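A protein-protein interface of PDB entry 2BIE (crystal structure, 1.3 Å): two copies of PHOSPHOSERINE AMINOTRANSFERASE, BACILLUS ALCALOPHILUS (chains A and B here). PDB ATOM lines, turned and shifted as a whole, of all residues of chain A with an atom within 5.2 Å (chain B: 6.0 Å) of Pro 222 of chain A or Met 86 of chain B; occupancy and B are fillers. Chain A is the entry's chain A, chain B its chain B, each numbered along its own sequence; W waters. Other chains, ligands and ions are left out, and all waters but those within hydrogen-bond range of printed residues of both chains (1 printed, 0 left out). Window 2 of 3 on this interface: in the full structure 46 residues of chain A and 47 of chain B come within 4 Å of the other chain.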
ATOM      1  N   GLN A 220     -26.916   8.316 -10.257  1.00  0.00           N
ATOM      2  CA  GLN A 220     -25.470   8.420 -10.251  1.00  0.00           C
ATOM      3  C   GLN A 220     -24.859   7.235 -10.958  1.00  0.00           C
ATOM      4  O   GLN A 220     -23.651   7.299 -11.168  1.00  0.00           O
ATOM      5  CB  GLN A 220     -24.907   8.497  -8.824  1.00  0.00           C
ATOM      6  CG  GLN A 220     -23.639   9.301  -8.655  1.00  0.00           C
ATOM      7  CD  GLN A 220     -23.883  10.798  -8.631  1.00  0.00           C
ATOM      8  OE1 GLN A 220     -24.921  11.265  -9.109  1.00  0.00           O
ATOM      9  NE2 GLN A 220     -22.938  11.555  -8.081  1.00  0.00           N
ATOM     10  N   VAL A 221     -25.610   6.199 -11.309  1.00  0.00           N
ATOM     11  CA  VAL A 221     -24.950   5.009 -11.851  1.00  0.00           C
ATOM     12  C   VAL A 221     -24.910   5.133 -13.367  1.00  0.00           C
ATOM     13  O   VAL A 221     -25.935   5.457 -13.954  1.00  0.00           O
ATOM     14  CB  VAL A 221     -25.703   3.745 -11.424  1.00  0.00           C
ATOM     15  CG1 VAL A 221     -25.153   2.509 -12.130  1.00  0.00           C
ATOM     16  CG2 VAL A 221     -25.635   3.552  -9.900  1.00  0.00           C
ATOM     17  N   PRO A 222     -23.764   4.936 -14.005  1.00  0.00           N
ATOM     18  CA  PRO A 222     -23.686   4.999 -15.466  1.00  0.00           C
ATOM     19  C   PRO A 222     -24.738   4.133 -16.146  1.00  0.00           C
ATOM     20  O   PRO A 222     -25.103   3.055 -15.661  1.00  0.00           O
ATOM     21  CB  PRO A 222     -22.298   4.426 -15.736  1.00  0.00           C
ATOM     22  CG  PRO A 222     -21.501   4.798 -14.523  1.00  0.00           C
ATOM     23  CD  PRO A 222     -22.468   4.691 -13.384  1.00  0.00           C
ATOM     24  N   THR A 223     -25.204   4.640 -17.286  1.00  0.00           N
ATOM     25  CA  THR A 223     -26.276   3.982 -18.031  1.00  0.00           C
ATOM     26  C   THR A 223     -26.069   2.490 -18.218  1.00  0.00           C
ATOM     27  O   THR A 223     -26.977   1.658 -17.972  1.00  0.00           O
ATOM     28  CB  THR A 223     -26.407   4.705 -19.399  1.00  0.00           C
ATOM     29  OG1 THR A 223     -26.509   6.112 -19.153  1.00  0.00           O
ATOM     30  CG2 THR A 223     -27.677   4.185 -20.056  1.00  0.00           C
ATOM     31  N   MET A 224     -24.885   2.106 -18.671  1.00  0.00           N
ATOM     32  CA  MET A 224     -24.624   0.695 -18.982  1.00  0.00           C
ATOM     33  C   MET A 224     -24.581  -0.167 -17.736  1.00  0.00           C
ATOM     34  O   MET A 224     -24.712  -1.396 -17.881  1.00  0.00           O
ATOM     35  CB  MET A 224     -23.311   0.522 -19.762  1.00  0.00           C
ATOM     36  CG  MET A 224     -23.333   0.754 -21.246  1.00  0.00           C
ATOM     37  SD  MET A 224     -24.298  -0.499 -22.116  1.00  0.00           S
ATOM     38  CE  MET A 224     -23.267  -1.965 -21.968  1.00  0.00           C
ATOM     39  N   LEU A 225     -24.423   0.451 -16.583  1.00  0.00           N
ATOM     40  CA  LEU A 225     -24.267  -0.301 -15.351  1.00  0.00           C
ATOM     41  C   LEU A 225     -25.534  -0.345 -14.517  1.00  0.00           C
ATOM     42  O   LEU A 225     -25.495  -0.930 -13.432  1.00  0.00           O
ATOM     43  CB  LEU A 225     -23.087   0.262 -14.528  1.00  0.00           C
ATOM     44  CG  LEU A 225     -21.727   0.010 -15.185  1.00  0.00           C
ATOM     45  CD1 LEU A 225     -20.746   0.966 -14.591  1.00  0.00           C
ATOM     46  CD2 LEU A 225     -21.398  -1.453 -14.938  1.00  0.00           C
ATOM     47  N   GLN A 226     -26.606   0.218 -15.000  1.00  0.00           N
ATOM     48  CA  GLN A 226     -27.924   0.087 -14.367  1.00  0.00           C
ATOM     49  C   GLN A 226     -28.679  -1.115 -14.876  1.00  0.00           C
ATOM     50  O   GLN A 226     -28.796  -1.269 -16.086  1.00  0.00           O
ATOM     51  CB  GLN A 226     -28.774   1.320 -14.707  1.00  0.00           C
ATOM     52  CG  GLN A 226     -28.171   2.579 -14.149  1.00  0.00           C
ATOM     53  CD  GLN A 226     -29.177   3.686 -14.082  1.00  0.00           C
ATOM     54  OE1 GLN A 226     -30.384   3.418 -14.168  1.00  0.00           O
ATOM     55  NE2 GLN A 226     -28.587   4.841 -13.905  1.00  0.00           N
ATOM     56  N   THR B  82     -18.391   5.207 -20.443  1.00  0.00           N
ATOM     57  CA  THR B  82     -18.227   5.448 -19.009  1.00  0.00           C
ATOM     58  C   THR B  82     -16.867   5.025 -18.483  1.00  0.00           C
ATOM     59  O   THR B  82     -16.321   5.711 -17.600  1.00  0.00           O
ATOM     60  CB  THR B  82     -19.411   4.800 -18.261  1.00  0.00           C
ATOM     61  OG1 THR B  82     -19.321   5.226 -16.874  1.00  0.00           O
ATOM     62  CG2 THR B  82     -19.363   3.306 -18.166  1.00  0.00           C
ATOM     63  N   MET B  83     -16.287   3.941 -18.987  1.00  0.00           N
ATOM     64  CA  MET B  83     -15.018   3.503 -18.405  1.00  0.00           C
ATOM     65  C   MET B  83     -13.936   4.551 -18.594  1.00  0.00           C
ATOM     66  O   MET B  83     -13.047   4.729 -17.732  1.00  0.00           O
ATOM     67  CB  MET B  83     -14.640   2.173 -19.049  1.00  0.00           C
ATOM     68  CG  MET B  83     -13.570   1.411 -18.326  1.00  0.00           C
ATOM     69  SD  MET B  83     -13.451  -0.276 -19.000  1.00  0.00           S
ATOM     70  CE  MET B  83     -11.905  -0.781 -18.262  1.00  0.00           C
ATOM     71  N   LEU B  84     -13.942   5.262 -19.708  1.00  0.00           N
ATOM     72  CA  LEU B  84     -12.890   6.264 -19.944  1.00  0.00           C
ATOM     73  C   LEU B  84     -12.961   7.339 -18.879  1.00  0.00           C
ATOM     74  O   LEU B  84     -11.957   7.559 -18.197  1.00  0.00           O
ATOM     75  CB  LEU B  84     -13.007   6.817 -21.347  1.00  0.00           C
ATOM     76  CG  LEU B  84     -12.362   8.179 -21.652  1.00  0.00           C
ATOM     77  CD1 LEU B  84     -10.896   7.912 -21.610  1.00  0.00           C
ATOM     78  CD2 LEU B  84     -12.832   8.745 -22.987  1.00  0.00           C
ATOM     79  N   PRO B  85     -14.048   8.061 -18.702  1.00  0.00           N
ATOM     80  CA  PRO B  85     -14.037   9.090 -17.644  1.00  0.00           C
ATOM     81  C   PRO B  85     -13.869   8.485 -16.271  1.00  0.00           C
ATOM     82  O   PRO B  85     -13.289   9.121 -15.404  1.00  0.00           O
ATOM     83  CB  PRO B  85     -15.386   9.818 -17.788  1.00  0.00           C
ATOM     84  CG  PRO B  85     -16.248   8.855 -18.541  1.00  0.00           C
ATOM     85  CD  PRO B  85     -15.313   8.138 -19.448  1.00  0.00           C
ATOM     86  N   MET B  86     -14.331   7.279 -16.052  1.00  0.00           N
ATOM     87  CA  MET B  86     -14.164   6.701 -14.739  1.00  0.00           C
ATOM     88  C   MET B  86     -12.686   6.579 -14.398  1.00  0.00           C
ATOM     89  O   MET B  86     -12.331   6.635 -13.219  1.00  0.00           O
ATOM     90  CB  MET B  86     -14.888   5.363 -14.715  1.00  0.00           C
ATOM     91  CG  MET B  86     -15.228   4.900 -13.322  1.00  0.00           C
ATOM     92  SD  MET B  86     -16.133   3.336 -13.283  1.00  0.00           S
ATOM     93  CE  MET B  86     -17.760   3.858 -13.885  1.00  0.00           C
ATOM     94  N   ASN B  87     -11.847   6.377 -15.385  1.00  0.00           N
ATOM     95  CA  ASN B  87     -10.411   6.232 -15.129  1.00  0.00           C
ATOM     96  C   ASN B  87      -9.696   7.554 -15.256  1.00  0.00           C
ATOM     97  O   ASN B  87      -8.730   7.742 -14.533  1.00  0.00           O
ATOM     98  CB  ASN B  87      -9.767   5.220 -16.068  1.00  0.00           C
ATOM     99  CG  ASN B  87     -10.044   3.780 -15.733  1.00  0.00           C
ATOM    100  OD1 ASN B  87      -9.164   3.069 -15.236  1.00  0.00           O
ATOM    101  ND2 ASN B  87     -11.271   3.335 -16.000  1.00  0.00           N
ATOM    102  N   LEU B  88     -10.085   8.452 -16.152  1.00  0.00           N
ATOM    103  CA  LEU B  88      -9.233   9.597 -16.430  1.00  0.00           C
ATOM    104  C   LEU B  88      -9.848  10.914 -15.998  1.00  0.00           C
ATOM    105  O   LEU B  88      -9.086  11.893 -15.891  1.00  0.00           O
ATOM    106  CB  LEU B  88      -8.933   9.583 -17.941  1.00  0.00           C
ATOM    107  CG  LEU B  88      -7.655  10.212 -18.451  1.00  0.00           C
ATOM    108  CD1 LEU B  88      -6.439   9.507 -17.853  1.00  0.00           C
ATOM    109  CD2 LEU B  88      -7.542  10.154 -19.972  1.00  0.00           C
ATOM    110  N   LEU B  89     -11.156  10.986 -15.791  1.00  0.00           N
ATOM    111  CA  LEU B  89     -11.774  12.277 -15.457  1.00  0.00           C
ATOM    112  C   LEU B  89     -11.714  12.468 -13.960  1.00  0.00           C
ATOM    113  O   LEU B  89     -12.658  12.133 -13.278  1.00  0.00           O
ATOM    114  CB  LEU B  89     -13.220  12.328 -15.975  1.00  0.00           C
ATOM    115  CG  LEU B  89     -13.989  13.644 -15.817  1.00  0.00           C
ATOM    116  CD1 LEU B  89     -13.156  14.821 -16.311  1.00  0.00           C
ATOM    117  CD2 LEU B  89     -15.322  13.527 -16.546  1.00  0.00           C
ATOM    118  N   GLU B 110     -22.251  10.287 -20.827  1.00  0.00           N
ATOM    119  CA  GLU B 110     -21.757   9.458 -19.729  1.00  0.00           C
ATOM    120  C   GLU B 110     -20.684  10.163 -18.911  1.00  0.00           C
ATOM    121  O   GLU B 110     -20.587   9.983 -17.718  1.00  0.00           O
ATOM    122  CB  GLU B 110     -21.180   8.148 -20.289  1.00  0.00           C
ATOM    123  CG  GLU B 110     -22.231   7.261 -20.893  1.00  0.00           C
ATOM    124  CD  GLU B 110     -23.420   7.017 -19.985  1.00  0.00           C
ATOM    125  OE1 GLU B 110     -23.193   6.611 -18.819  1.00  0.00           O
ATOM    126  OE2 GLU B 110     -24.558   7.209 -20.484  1.00  0.00           O
ATOM    127  N   LEU B 113     -21.977  12.443 -16.021  1.00  0.00           N
ATOM    128  CA  LEU B 113     -22.338  11.820 -14.770  1.00  0.00           C
ATOM    129  C   LEU B 113     -21.162  11.736 -13.807  1.00  0.00           C
ATOM    130  O   LEU B 113     -21.349  11.564 -12.604  1.00  0.00           O
ATOM    131  CB  LEU B 113     -22.810  10.384 -15.057  1.00  0.00           C
ATOM    132  CG  LEU B 113     -24.176  10.260 -15.700  1.00  0.00           C
ATOM    133  CD1 LEU B 113     -24.522   8.859 -16.235  1.00  0.00           C
ATOM    134  CD2 LEU B 113     -25.264  10.647 -14.688  1.00  0.00           C
ATOM    135  N   LEU B 114     -19.951  11.824 -14.353  1.00  0.00           N
ATOM    136  CA  LEU B 114     -18.783  11.566 -13.529  1.00  0.00           C
ATOM    137  C   LEU B 114     -17.888  12.750 -13.250  1.00  0.00           C
ATOM    138  O   LEU B 114     -17.039  12.668 -12.355  1.00  0.00           O
ATOM    139  CB  LEU B 114     -17.982  10.484 -14.233  1.00  0.00           C
ATOM    140  CG  LEU B 114     -18.837   9.226 -14.514  1.00  0.00           C
ATOM    141  CD1 LEU B 114     -17.963   8.206 -15.235  1.00  0.00           C
ATOM    142  CD2 LEU B 114     -19.483   8.665 -13.278  1.00  0.00           C
ATOM    143  N   VAL B 218      -6.038   3.691  -9.801  1.00  0.00           N
ATOM    144  CA  VAL B 218      -7.328   4.408  -9.730  1.00  0.00           C
ATOM    145  C   VAL B 218      -8.239   3.776  -8.675  1.00  0.00           C
ATOM    146  O   VAL B 218      -9.237   3.078  -8.809  1.00  0.00           O
ATOM    147  CB  VAL B 218      -7.983   4.577 -11.119  1.00  0.00           C
ATOM    148  CG1 VAL B 218      -8.580   3.308 -11.683  1.00  0.00           C
ATOM    149  CG2 VAL B 218      -9.033   5.686 -11.020  1.00  0.00           C
ATOM    150  N   VAL B 221     -12.099   2.710  -8.050  1.00  0.00           N
ATOM    151  CA  VAL B 221     -12.810   2.209  -9.241  1.00  0.00           C
ATOM    152  C   VAL B 221     -12.941   0.697  -9.166  1.00  0.00           C
ATOM    153  O   VAL B 221     -11.945   0.001  -8.863  1.00  0.00           O
ATOM    154  CB  VAL B 221     -12.061   2.646 -10.511  1.00  0.00           C
ATOM    155  CG1 VAL B 221     -12.666   2.088 -11.783  1.00  0.00           C
ATOM    156  CG2 VAL B 221     -12.001   4.172 -10.569  1.00  0.00           C
ATOM    157  N   PRO B 222     -14.124   0.142  -9.420  1.00  0.00           N
ATOM    158  CA  PRO B 222     -14.253  -1.329  -9.442  1.00  0.00           C
ATOM    159  C   PRO B 222     -13.212  -2.000 -10.294  1.00  0.00           C
ATOM    160  O   PRO B 222     -12.861  -1.514 -11.364  1.00  0.00           O
ATOM    161  CB  PRO B 222     -15.649  -1.524 -10.009  1.00  0.00           C
ATOM    162  CG  PRO B 222     -16.394  -0.325  -9.531  1.00  0.00           C
ATOM    163  CD  PRO B 222     -15.413   0.805  -9.633  1.00  0.00           C
ATOM    164  N   LEU B 225     -13.533  -2.356 -14.014  1.00  0.00           N
ATOM    165  CA  LEU B 225     -13.658  -1.063 -14.722  1.00  0.00           C
ATOM    166  C   LEU B 225     -12.379  -0.268 -14.692  1.00  0.00           C
ATOM    167  O   LEU B 225     -12.357   0.828 -15.238  1.00  0.00           O
ATOM    168  CB  LEU B 225     -14.838  -0.284 -14.114  1.00  0.00           C
ATOM    169  CG  LEU B 225     -16.194  -0.925 -14.423  1.00  0.00           C
ATOM    170  CD1 LEU B 225     -17.311  -0.421 -13.521  1.00  0.00           C
ATOM    171  CD2 LEU B 225     -16.542  -0.727 -15.903  1.00  0.00           C
HETATM  172  O   HOH W   1     -22.725   3.867 -19.386  1.00  0.00           O
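Leu 225 of chain B touches its own counterpart, Leu 225 of chain A.
The side-chain amide nitrogen (ND2) of Asn 87 of chain B lies within hydrogen-bond range of the backbone carbonyl oxygen (O) of Leu 225 of chain B, 2.8 Å away.
Water W1 lies within hydrogen-bond range of the side-chain carboxylate (OE1) of Glu 110 of chain B (2.8 Å), the backbone NH (N) of Met 224 of chain A (2.9 Å) and the backbone NH (N) of Thr 223 of chain A (3.3 Å).
Printed residues of chain B that touch a printed residue of chain A: Thr 82, Met 86, Glu 110 and Leu 225. Hydrophobic or aromatic side chains of chain B that line the printed part of chain A: Met 86 and Leu 225. Of the 7 printed residues of chain A, 3 touch a printed residue of chain B. Hydrophobic or aromatic side chains of chain A within 4 Å of the printed part of chain B: Pro 222 and Leu 225. Among the printed residues, 5 pairs touch across the chains. Among the printed residues, no Asp or Glu carboxylate lies within 4 Å of a Lys or Arg side-chain nitrogen of the other chain.
Among the printed residues, merely in contact across the chains: Pro 222 of chain A with Thr 82 of chain B, Pro 222 of chain A with Glu 110 of chain B, Leu 225 of chain A with Leu 225 of chain B and Pro 222 of chain A with Met 86 of chain B.
The side-chain hydroxyl of Thr 223 of chain A is in hydrogen-bond range of the side-chain carboxylate of Glu 110 of chain B.
Printed residues of chain A within 4 Å of Met 86 of chain B: Pro 222. Printed residues of chain A within 4 Å of Thr 82 of chain B: Pro 222. Of the printed residues of chain A, Leu 225 of chain B touches Leu 225. Printed residues of chain A within 4 Å of Glu 110 of chain B: Pro 222 and Thr 223. Printed residues of chain B within 4 Å of Leu 225 of chain A: Leu 225 (3.9 Å). Of the printed residues of chain B, Thr 223 of chain A touches Glu 110. The nearest printed residue of chain A that does not touch Met 86 of chain B is Leu 225 of chain A (4.2 Å). The nearest printed residue of chain A that does not touch Thr 82 of chain B is Leu 225 of chain A (4.5 Å).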
